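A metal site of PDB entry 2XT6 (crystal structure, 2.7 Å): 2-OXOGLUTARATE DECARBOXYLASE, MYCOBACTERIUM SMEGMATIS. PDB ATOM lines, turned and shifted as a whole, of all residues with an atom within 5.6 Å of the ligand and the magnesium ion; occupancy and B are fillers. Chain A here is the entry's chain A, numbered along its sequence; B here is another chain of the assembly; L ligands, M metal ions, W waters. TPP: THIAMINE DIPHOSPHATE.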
ATOM      1  N   HIS A 425      17.046  -2.374  -7.768  1.00  0.00           N
ATOM      2  CA  HIS A 425      17.584  -3.470  -8.587  1.00  0.00           C
ATOM      3  C   HIS A 425      18.762  -4.222  -7.925  1.00  0.00           C
ATOM      4  O   HIS A 425      18.921  -5.421  -8.196  1.00  0.00           O
ATOM      5  CB  HIS A 425      18.053  -2.923  -9.953  1.00  0.00           C
ATOM      6  CG  HIS A 425      19.085  -1.834  -9.835  1.00  0.00           C
ATOM      7  ND1 HIS A 425      20.402  -2.032 -10.250  1.00  0.00           N
ATOM      8  CD2 HIS A 425      18.963  -0.577  -9.350  1.00  0.00           C
ATOM      9  CE1 HIS A 425      21.033  -0.894 -10.009  1.00  0.00           C
ATOM     10  NE2 HIS A 425      20.212   0.004  -9.449  1.00  0.00           N
ATOM     11  N   ARG A 426      19.589  -3.532  -7.091  1.00  0.00           N
ATOM     12  CA  ARG A 426      20.764  -4.133  -6.441  1.00  0.00           C
ATOM     13  C   ARG A 426      20.420  -5.388  -5.611  1.00  0.00           C
ATOM     14  O   ARG A 426      19.806  -5.290  -4.529  1.00  0.00           O
ATOM     15  CB  ARG A 426      21.556  -3.131  -5.579  1.00  0.00           C
ATOM     16  CG  ARG A 426      22.950  -3.660  -5.238  1.00  0.00           C
ATOM     17  CD  ARG A 426      23.867  -2.681  -4.512  1.00  0.00           C
ATOM     18  NE  ARG A 426      24.187  -1.482  -5.287  1.00  0.00           N
ATOM     19  CZ  ARG A 426      25.045  -1.413  -6.296  1.00  0.00           C
ATOM     20  NH1 ARG A 426      25.698  -2.494  -6.706  1.00  0.00           N
ATOM     21  NH2 ARG A 426      25.264  -0.258  -6.913  1.00  0.00           N
ATOM     22  N   SER A 490      12.902   2.284 -12.406  1.00  0.00           N
ATOM     23  CA  SER A 490      14.285   2.615 -12.109  1.00  0.00           C
ATOM     24  C   SER A 490      14.324   3.849 -11.219  1.00  0.00           C
ATOM     25  O   SER A 490      15.378   4.139 -10.652  1.00  0.00           O
ATOM     26  CB  SER A 490      15.084   2.819 -13.393  1.00  0.00           C
ATOM     27  OG  SER A 490      15.112   1.626 -14.158  1.00  0.00           O
ATOM     28  N   HIS A 491      13.185   4.566 -11.072  1.00  0.00           N
ATOM     29  CA  HIS A 491      13.023   5.729 -10.172  1.00  0.00           C
ATOM     30  C   HIS A 491      13.077   5.262  -8.758  1.00  0.00           C
ATOM     31  O   HIS A 491      12.112   4.644  -8.263  1.00  0.00           O
ATOM     32  CB  HIS A 491      11.699   6.448 -10.422  1.00  0.00           C
ATOM     33  CG  HIS A 491      11.654   7.118 -11.737  1.00  0.00           C
ATOM     34  ND1 HIS A 491      11.888   6.425 -12.909  1.00  0.00           N
ATOM     35  CD2 HIS A 491      11.382   8.415 -12.032  1.00  0.00           C
ATOM     36  CE1 HIS A 491      11.806   7.329 -13.872  1.00  0.00           C
ATOM     37  NE2 HIS A 491      11.481   8.531 -13.378  1.00  0.00           N
ATOM     38  N   LEU A 492      14.232   5.494  -8.110  1.00  0.00           N
ATOM     39  CA  LEU A 492      14.532   5.054  -6.752  1.00  0.00           C
ATOM     40  C   LEU A 492      13.539   5.602  -5.741  1.00  0.00           C
ATOM     41  O   LEU A 492      13.137   6.781  -5.798  1.00  0.00           O
ATOM     42  CB  LEU A 492      15.982   5.419  -6.360  1.00  0.00           C
ATOM     43  CG  LEU A 492      17.072   4.719  -7.209  1.00  0.00           C
ATOM     44  CD1 LEU A 492      18.389   5.461  -7.141  1.00  0.00           C
ATOM     45  CD2 LEU A 492      17.246   3.277  -6.824  1.00  0.00           C
ATOM     46  N   GLY A 530      18.808   2.155  -0.814  1.00  0.00           N
ATOM     47  CA  GLY A 530      20.236   2.431  -0.909  1.00  0.00           C
ATOM     48  C   GLY A 530      20.457   3.663  -0.069  1.00  0.00           C
ATOM     49  O   GLY A 530      19.505   4.406   0.194  1.00  0.00           O
ATOM     50  N   ASP A 531      21.711   3.901   0.359  1.00  0.00           N
ATOM     51  CA  ASP A 531      22.032   5.027   1.246  1.00  0.00           C
ATOM     52  C   ASP A 531      21.773   6.416   0.639  1.00  0.00           C
ATOM     53  O   ASP A 531      21.203   7.264   1.325  1.00  0.00           O
ATOM     54  CB  ASP A 531      23.473   4.936   1.774  1.00  0.00           C
ATOM     55  CG  ASP A 531      24.618   5.009   0.788  1.00  0.00           C
ATOM     56  OD1 ASP A 531      24.734   4.091  -0.046  1.00  0.00           O
ATOM     57  OD2 ASP A 531      25.498   5.918   0.964  1.00  0.00           O
ATOM     58  N   ALA A 532      22.177   6.657  -0.626  1.00  0.00           N
ATOM     59  CA  ALA A 532      21.976   7.985  -1.237  1.00  0.00           C
ATOM     60  C   ALA A 532      20.485   8.313  -1.535  1.00  0.00           C
ATOM     61  O   ALA A 532      20.050   9.424  -1.269  1.00  0.00           O
ATOM     62  CB  ALA A 532      22.791   8.111  -2.496  1.00  0.00           C
ATOM     63  N   ALA A 533      19.713   7.334  -2.051  1.00  0.00           N
ATOM     64  CA  ALA A 533      18.322   7.515  -2.401  1.00  0.00           C
ATOM     65  C   ALA A 533      17.458   7.727  -1.148  1.00  0.00           C
ATOM     66  O   ALA A 533      16.607   8.619  -1.132  1.00  0.00           O
ATOM     67  CB  ALA A 533      17.842   6.323  -3.217  1.00  0.00           C
ATOM     68  N   PHE A 534      17.737   6.973  -0.061  1.00  0.00           N
ATOM     69  CA  PHE A 534      16.983   7.095   1.191  1.00  0.00           C
ATOM     70  C   PHE A 534      17.082   8.507   1.785  1.00  0.00           C
ATOM     71  O   PHE A 534      16.085   9.013   2.308  1.00  0.00           O
ATOM     72  CB  PHE A 534      17.462   6.050   2.225  1.00  0.00           C
ATOM     73  CG  PHE A 534      16.512   5.844   3.381  1.00  0.00           C
ATOM     74  CD1 PHE A 534      15.350   5.091   3.227  1.00  0.00           C
ATOM     75  CD2 PHE A 534      16.782   6.409   4.629  1.00  0.00           C
ATOM     76  CE1 PHE A 534      14.484   4.892   4.307  1.00  0.00           C
ATOM     77  CE2 PHE A 534      15.888   6.226   5.702  1.00  0.00           C
ATOM     78  CZ  PHE A 534      14.757   5.469   5.539  1.00  0.00           C
ATOM     79  N   GLN A 537      15.676  11.418  -1.505  1.00  0.00           N
ATOM     80  CA  GLN A 537      14.323  11.366  -2.097  1.00  0.00           C
ATOM     81  C   GLN A 537      13.208  11.686  -1.078  1.00  0.00           C
ATOM     82  O   GLN A 537      13.054  10.970  -0.087  1.00  0.00           O
ATOM     83  CB  GLN A 537      14.072  10.013  -2.779  1.00  0.00           C
ATOM     84  CG  GLN A 537      14.900   9.768  -4.049  1.00  0.00           C
ATOM     85  CD  GLN A 537      14.407  10.500  -5.267  1.00  0.00           C
ATOM     86  OE1 GLN A 537      13.281  10.304  -5.726  1.00  0.00           O
ATOM     87  NE2 GLN A 537      15.259  11.331  -5.850  1.00  0.00           N
ATOM     88  N   VAL A 562      20.772  -0.744   2.497  1.00  0.00           N
ATOM     89  CA  VAL A 562      22.017  -1.346   2.009  1.00  0.00           C
ATOM     90  C   VAL A 562      22.956  -0.133   1.790  1.00  0.00           C
ATOM     91  O   VAL A 562      22.960   0.487   0.731  1.00  0.00           O
ATOM     92  CB  VAL A 562      21.779  -2.212   0.740  1.00  0.00           C
ATOM     93  CG1 VAL A 562      23.075  -2.841   0.232  1.00  0.00           C
ATOM     94  CG2 VAL A 562      20.704  -3.288   0.985  1.00  0.00           C
ATOM     95  N   ASN A 563      23.594   0.286   2.882  1.00  0.00           N
ATOM     96  CA  ASN A 563      24.467   1.454   2.936  1.00  0.00           C
ATOM     97  C   ASN A 563      25.928   1.069   2.621  1.00  0.00           C
ATOM     98  O   ASN A 563      26.718   0.775   3.529  1.00  0.00           O
ATOM     99  CB  ASN A 563      24.326   2.045   4.326  1.00  0.00           C
ATOM    100  CG  ASN A 563      25.175   3.222   4.672  1.00  0.00           C
ATOM    101  OD1 ASN A 563      25.823   3.861   3.837  1.00  0.00           O
ATOM    102  ND2 ASN A 563      25.157   3.555   5.953  1.00  0.00           N
ATOM    103  N   ASN A 564      26.282   1.078   1.315  1.00  0.00           N
ATOM    104  CA  ASN A 564      27.617   0.770   0.808  1.00  0.00           C
ATOM    105  C   ASN A 564      28.512   2.028   0.803  1.00  0.00           C
ATOM    106  O   ASN A 564      29.554   2.051   0.152  1.00  0.00           O
ATOM    107  CB  ASN A 564      27.524   0.152  -0.574  1.00  0.00           C
ATOM    108  CG  ASN A 564      26.574   0.801  -1.548  1.00  0.00           C
ATOM    109  OD1 ASN A 564      26.227   1.977  -1.451  1.00  0.00           O
ATOM    110  ND2 ASN A 564      26.189   0.056  -2.573  1.00  0.00           N
ATOM    111  N   GLN A 565      28.098   3.077   1.555  1.00  0.00           N
ATOM    112  CA  GLN A 565      28.806   4.337   1.793  1.00  0.00           C
ATOM    113  C   GLN A 565      29.250   5.075   0.463  1.00  0.00           C
ATOM    114  O   GLN A 565      30.254   5.805   0.412  1.00  0.00           O
ATOM    115  CB  GLN A 565      30.016   4.037   2.697  1.00  0.00           C
ATOM    116  CG  GLN A 565      29.664   3.182   3.909  1.00  0.00           C
ATOM    117  CD  GLN A 565      30.874   2.772   4.703  1.00  0.00           C
ATOM    118  OE1 GLN A 565      31.602   3.621   5.235  1.00  0.00           O
ATOM    119  NE2 GLN A 565      31.089   1.466   4.823  1.00  0.00           N
ATOM    120  N   ILE A 566      28.428   4.883  -0.590  1.00  0.00           N
ATOM    121  CA  ILE A 566      28.648   5.396  -1.943  1.00  0.00           C
ATOM    122  C   ILE A 566      27.300   5.450  -2.707  1.00  0.00           C
ATOM    123  O   ILE A 566      26.422   4.600  -2.505  1.00  0.00           O
ATOM    124  CB  ILE A 566      29.723   4.510  -2.699  1.00  0.00           C
ATOM    125  CG1 ILE A 566      30.310   5.187  -3.970  1.00  0.00           C
ATOM    126  CG2 ILE A 566      29.268   3.067  -3.008  1.00  0.00           C
ATOM    127  CD1 ILE A 566      31.297   6.173  -3.698  1.00  0.00           C
ATOM    128  N   GLY A 567      27.197   6.444  -3.591  1.00  0.00           N
ATOM    129  CA  GLY A 567      26.046   6.651  -4.459  1.00  0.00           C
ATOM    130  C   GLY A 567      26.577   6.911  -5.856  1.00  0.00           C
ATOM    131  O   GLY A 567      26.827   8.066  -6.225  1.00  0.00           O
ATOM    132  N   PHE A 568      26.800   5.813  -6.616  1.00  0.00           N
ATOM    133  CA  PHE A 568      27.384   5.819  -7.964  1.00  0.00           C
ATOM    134  C   PHE A 568      28.844   6.350  -7.897  1.00  0.00           C
ATOM    135  O   PHE A 568      29.777   5.570  -7.702  1.00  0.00           O
ATOM    136  CB  PHE A 568      26.501   6.599  -8.960  1.00  0.00           C
ATOM    137  CG  PHE A 568      26.821   6.485 -10.438  1.00  0.00           C
ATOM    138  CD1 PHE A 568      28.110   6.116 -10.861  1.00  0.00           C
ATOM    139  CD2 PHE A 568      25.874   6.800 -11.401  1.00  0.00           C
ATOM    140  CE1 PHE A 568      28.407   6.019 -12.224  1.00  0.00           C
ATOM    141  CE2 PHE A 568      26.189   6.750 -12.765  1.00  0.00           C
ATOM    142  CZ  PHE A 568      27.449   6.351 -13.177  1.00  0.00           C
ATOM    143  N   ARG A 629      30.566  -1.550  -1.876  1.00  0.00           N
ATOM    144  CA  ARG A 629      30.311  -1.936  -3.246  1.00  0.00           C
ATOM    145  C   ARG A 629      31.684  -2.301  -3.796  1.00  0.00           C
ATOM    146  O   ARG A 629      32.503  -1.396  -3.986  1.00  0.00           O
ATOM    147  CB  ARG A 629      29.656  -0.763  -3.976  1.00  0.00           C
ATOM    148  CG  ARG A 629      28.844  -1.145  -5.199  1.00  0.00           C
ATOM    149  CD  ARG A 629      28.622   0.073  -6.068  1.00  0.00           C
ATOM    150  NE  ARG A 629      29.907   0.650  -6.479  1.00  0.00           N
ATOM    151  CZ  ARG A 629      30.076   1.916  -6.827  1.00  0.00           C
ATOM    152  NH1 ARG A 629      29.054   2.746  -6.861  1.00  0.00           N
ATOM    153  NH2 ARG A 629      31.283   2.359  -7.146  1.00  0.00           N
ATOM    154  N   HIS A 633      30.245   0.984 -10.508  1.00  0.00           N
ATOM    155  CA  HIS A 633      28.813   1.163 -10.552  1.00  0.00           C
ATOM    156  C   HIS A 633      28.230   0.424 -11.722  1.00  0.00           C
ATOM    157  O   HIS A 633      27.181  -0.186 -11.565  1.00  0.00           O
ATOM    158  CB  HIS A 633      28.412   2.645 -10.605  1.00  0.00           C
ATOM    159  CG  HIS A 633      26.940   2.838 -10.382  1.00  0.00           C
ATOM    160  ND1 HIS A 633      26.382   2.749  -9.108  1.00  0.00           N
ATOM    161  CD2 HIS A 633      25.956   3.072 -11.283  1.00  0.00           C
ATOM    162  CE1 HIS A 633      25.075   2.941  -9.277  1.00  0.00           C
ATOM    163  NE2 HIS A 633      24.773   3.130 -10.570  1.00  0.00           N
ATOM    164  N   GLN B 787      23.510  14.863 -10.787  1.00  0.00           N
ATOM    165  CA  GLN B 787      23.970  13.599 -10.179  1.00  0.00           C
ATOM    166  C   GLN B 787      25.203  13.097 -10.907  1.00  0.00           C
ATOM    167  O   GLN B 787      25.156  12.886 -12.121  1.00  0.00           O
ATOM    168  CB  GLN B 787      22.860  12.552 -10.176  1.00  0.00           C
ATOM    169  CG  GLN B 787      21.956  12.620  -8.953  1.00  0.00           C
ATOM    170  CD  GLN B 787      20.528  12.334  -9.314  1.00  0.00           C
ATOM    171  OE1 GLN B 787      20.218  11.462 -10.129  1.00  0.00           O
ATOM    172  NE2 GLN B 787      19.609  13.065  -8.713  1.00  0.00           N
ATOM    173  N   ASP B 788      26.328  12.968 -10.164  1.00  0.00           N
ATOM    174  CA  ASP B 788      27.624  12.507 -10.670  1.00  0.00           C
ATOM    175  C   ASP B 788      28.097  13.377 -11.872  1.00  0.00           C
ATOM    176  O   ASP B 788      28.714  12.854 -12.796  1.00  0.00           O
ATOM    177  CB  ASP B 788      27.547  11.012 -11.035  1.00  0.00           C
ATOM    178  CG  ASP B 788      26.930  10.160  -9.934  1.00  0.00           C
ATOM    179  OD1 ASP B 788      27.595   9.951  -8.909  1.00  0.00           O
ATOM    180  OD2 ASP B 788      25.736   9.800 -10.067  1.00  0.00           O
ATOM    181  N   LEU B 836      20.834  12.914  -4.183  1.00  0.00           N
ATOM    182  CA  LEU B 836      19.966  12.115  -5.048  1.00  0.00           C
ATOM    183  C   LEU B 836      18.521  12.608  -4.974  1.00  0.00           C
ATOM    184  O   LEU B 836      17.635  11.946  -4.432  1.00  0.00           O
ATOM    185  CB  LEU B 836      20.060  10.610  -4.731  1.00  0.00           C
ATOM    186  CG  LEU B 836      20.079   9.686  -5.927  1.00  0.00           C
ATOM    187  CD1 LEU B 836      20.573   8.324  -5.535  1.00  0.00           C
ATOM    188  CD2 LEU B 836      18.715   9.593  -6.609  1.00  0.00           C
ATOM    189  N   GLU B 838      15.647  15.313  -7.465  1.00  0.00           N
ATOM    190  CA  GLU B 838      15.387  15.993  -8.743  1.00  0.00           C
ATOM    191  C   GLU B 838      14.630  17.283  -8.483  1.00  0.00           C
ATOM    192  O   GLU B 838      15.001  18.322  -9.002  1.00  0.00           O
ATOM    193  CB  GLU B 838      14.646  15.107  -9.762  1.00  0.00           C
ATOM    194  CG  GLU B 838      15.509  14.006 -10.361  1.00  0.00           C
ATOM    195  CD  GLU B 838      15.854  12.821  -9.470  1.00  0.00           C
ATOM    196  OE1 GLU B 838      16.995  12.299  -9.575  1.00  0.00           O
ATOM    197  OE2 GLU B 838      14.979  12.390  -8.677  1.00  0.00           O
ATOM    198  N   GLN B 862      20.576  12.623 -14.605  1.00  0.00           N
ATOM    199  CA  GLN B 862      21.409  11.437 -14.770  1.00  0.00           C
ATOM    200  C   GLN B 862      21.003  10.831 -16.132  1.00  0.00           C
ATOM    201  O   GLN B 862      21.841  10.577 -17.006  1.00  0.00           O
ATOM    202  CB  GLN B 862      21.202  10.492 -13.576  1.00  0.00           C
ATOM    203  CG  GLN B 862      21.982   9.189 -13.694  1.00  0.00           C
ATOM    204  CD  GLN B 862      22.984   9.048 -12.606  1.00  0.00           C
ATOM    205  OE1 GLN B 862      22.879   8.164 -11.777  1.00  0.00           O
ATOM    206  NE2 GLN B 862      23.998   9.904 -12.596  1.00  0.00           N
ATOM    207  N   PHE B 866      14.444  10.875 -15.376  1.00  0.00           N
ATOM    208  CA  PHE B 866      14.231  11.120 -13.961  1.00  0.00           C
ATOM    209  C   PHE B 866      13.765  12.544 -13.652  1.00  0.00           C
ATOM    210  O   PHE B 866      13.243  12.755 -12.538  1.00  0.00           O
ATOM    211  CB  PHE B 866      15.493  10.749 -13.154  1.00  0.00           C
ATOM    212  CG  PHE B 866      15.864   9.286 -13.338  1.00  0.00           C
ATOM    213  CD1 PHE B 866      17.066   8.917 -13.936  1.00  0.00           C
ATOM    214  CD2 PHE B 866      14.980   8.284 -12.945  1.00  0.00           C
ATOM    215  CE1 PHE B 866      17.383   7.577 -14.121  1.00  0.00           C
ATOM    216  CE2 PHE B 866      15.300   6.925 -13.167  1.00  0.00           C
ATOM    217  CZ  PHE B 866      16.506   6.588 -13.731  1.00  0.00           C
ATOM    218  N   HIS B 906      15.585   4.713 -19.227  1.00  0.00           N
ATOM    219  CA  HIS B 906      16.913   5.132 -19.696  1.00  0.00           C
ATOM    220  C   HIS B 906      16.823   5.453 -21.176  1.00  0.00           C
ATOM    221  O   HIS B 906      17.739   5.107 -21.925  1.00  0.00           O
ATOM    222  CB  HIS B 906      17.968   4.049 -19.385  1.00  0.00           C
ATOM    223  CG  HIS B 906      18.024   3.684 -17.929  1.00  0.00           C
ATOM    224  ND1 HIS B 906      18.809   4.421 -17.036  1.00  0.00           N
ATOM    225  CD2 HIS B 906      17.311   2.766 -17.230  1.00  0.00           C
ATOM    226  CE1 HIS B 906      18.588   3.887 -15.842  1.00  0.00           C
ATOM    227  NE2 HIS B 906      17.682   2.902 -15.916  1.00  0.00           N
HETATM  228  N1' TPP L   1      16.936   9.366  -9.667  1.00  0.00           N
HETATM  229  C2' TPP L   1      16.065   8.390  -9.449  1.00  0.00           C
HETATM  230  CM2 TPP L   1      14.725   8.624  -8.810  1.00  0.00           C
HETATM  231  N3' TPP L   1      16.342   7.159  -9.802  1.00  0.00           N
HETATM  232  C4' TPP L   1      17.491   6.841 -10.352  1.00  0.00           C
HETATM  233  N4' TPP L   1      17.640   5.521 -10.692  1.00  0.00           N
HETATM  234  C5' TPP L   1      18.475   7.831 -10.588  1.00  0.00           C
HETATM  235  C6' TPP L   1      18.133   9.127 -10.230  1.00  0.00           C
HETATM  236  C7' TPP L   1      19.839   7.503 -11.175  1.00  0.00           C
HETATM  237  N3  TPP L   1      20.625   6.585 -10.325  1.00  0.00           N
HETATM  238  C2  TPP L   1      20.722   5.313 -10.558  1.00  0.00           C
HETATM  239  S1  TPP L   1      21.776   4.524  -9.425  1.00  0.00           S
HETATM  240  C5  TPP L   1      22.035   6.071  -8.614  1.00  0.00           C
HETATM  241  C4  TPP L   1      21.324   7.001  -9.272  1.00  0.00           C
HETATM  242  CM4 TPP L   1      21.436   8.422  -8.814  1.00  0.00           C
HETATM  243  C6  TPP L   1      22.862   6.201  -7.359  1.00  0.00           C
HETATM  244  C7  TPP L   1      22.250   5.289  -6.284  1.00  0.00           C
HETATM  245  O7  TPP L   1      22.790   5.541  -4.982  1.00  0.00           O
HETATM  246  PA  TPP L   1      22.357   4.606  -3.741  1.00  0.00           P
HETATM  247  O1A TPP L   1      20.998   4.994  -3.307  1.00  0.00           O
HETATM  248  O2A TPP L   1      23.355   4.724  -2.497  1.00  0.00           O
HETATM  249  O3A TPP L   1      22.338   3.078  -4.238  1.00  0.00           O
HETATM  250  PB  TPP L   1      23.378   2.030  -4.574  1.00  0.00           P
HETATM  251  O1B TPP L   1      23.323   1.766  -6.164  1.00  0.00           O
HETATM  252  O2B TPP L   1      24.713   2.492  -4.165  1.00  0.00           O
HETATM  253  O3B TPP L   1      23.047   0.657  -3.782  1.00  0.00           O
HETATM  254 MG    MG M   1      24.714   3.327  -1.980  1.00  0.00          MG
HETATM  255  O   HOH W   1      26.287   2.967  -6.281  1.00  0.00           O
HETATM  256  O   HOH W   2      23.434   1.874  -1.405  1.00  0.00           O
HETATM  257  O   HOH W   3      19.171   3.758 -12.939  1.00  0.00           O
HETATM  258  O   HOH W   4      19.061   2.863  -4.033  1.00  0.00           O
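S1 of the ligand lies close to NE2 of His 633, at 3.5 Å.
O3B of the ligand is in salt-bridge range of NE of Arg 426 (2.9 Å).
N4' of the ligand is in hydrogen-bond range of O of Ser 490.
N of Ala 532 is in hydrogen-bond range of O1A of the ligand, at 3.4 Å.
The backbone NH of Ala 533 is in hydrogen-bond range of an oxygen (O1A) of the ligand, 3.0 Å away.
O2A of the ligand sits close to N of Asp 531 (3.4 Å).
The backbone NH (N) of Leu 492 is in hydrogen-bond range of a nitrogen (N3') of the ligand, at 3.2 Å.
The side-chain amide nitrogen (NE2) of Gln 862 of chain B is in hydrogen-bond range of the side-chain carboxylate (OD2) of Asp 788 of chain B, 3.1 Å away.
NH1 of Arg 629 sits at hydrogen-bond distance from ND1 of His 633 (3.5 Å).
The side-chain hydroxyl (OG) of Ser 490 is in hydrogen-bond range of a ring nitrogen (NE2) of His 906 of chain B (3.4 Å).
NE2 of Gln 787 of chain B sits at hydrogen-bond distance from OE1 of Glu 838 of chain B (2.9 Å).
NE2 of Gln 537 is in hydrogen-bond range of O of Leu 836 of chain B, at 2.8 Å.
NH1 of Arg 629 lies within hydrogen-bond range of O of Phe 568, at 3.0 Å.
The side-chain amide nitrogen (NE2) of Gln 862 of chain B sits at hydrogen-bond distance from the backbone carbonyl oxygen (O) of Gln 787 of chain B.
The side-chain carboxylate (OE2) of Glu 838 of chain B lies within hydrogen-bond range of the side-chain amide nitrogen (NE2) of Gln 537 (3.0 Å).
A nitrogen (N1') of the ligand sits close to the side-chain carboxylate (OE1) of Glu 838 of chain B (2.9 Å).
N3 of the ligand sits close to OE1 of Gln 862 of chain B.
Merely in contact with the ligand: His 491 (3.6 Å), Gly 530 (3.5 Å), Gln 537 (3.8 Å), Gly 567 (3.5 Å), Phe 568 (3.995 Å), Gln 787 of chain B (3.1 Å), Leu 836 of chain B (3.4 Å) and Phe 866 of chain B (3.4 Å).
Hydrophobic or aromatic side chains within 4 Å of the ligand: Leu 492, Ala 532, Ala 533, Phe 568, His 633, Leu 836 of chain B and Phe 866 of chain B.
Of the 27 residues printed, 19 come within 4 Å of the ligand.
The nearest printed residue that does not touch the ligand is Val 562 (4.5 Å).
Water W2 lies within hydrogen-bond range of O of Val 562 (2.6 Å), O3B of the ligand (2.7 Å) and N of Asp 531 (3.2 Å).
Water W4 lies within hydrogen-bond range of O1A of the ligand (3.0 Å) and N of Gly 530 (3.3 Å).
Water W3 lies within hydrogen-bond range of N4' of the ligand and NE2 of His 906 of chain B.
O2A of the ligand binds the magnesium ion (2.0 Å).
Water W2 is bound to the magnesium ion, 2.0 Å away.
OD1 of Asp 531 binds the magnesium ion (2.1 Å).
OD1 of Asn 564 binds the magnesium ion (2.1 Å).
O of Ile 566 binds the magnesium ion (2.2 Å).
O2B of the ligand binds the magnesium ion, 2.3 Å away.
The magnesium ion has six donor atoms within binding distance.
Of the 27 residues printed, 3 come within 4 Å of the magnesium ion.
The nearest printed residue that does not touch the magnesium ion is Gly 567 (4.3 Å).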
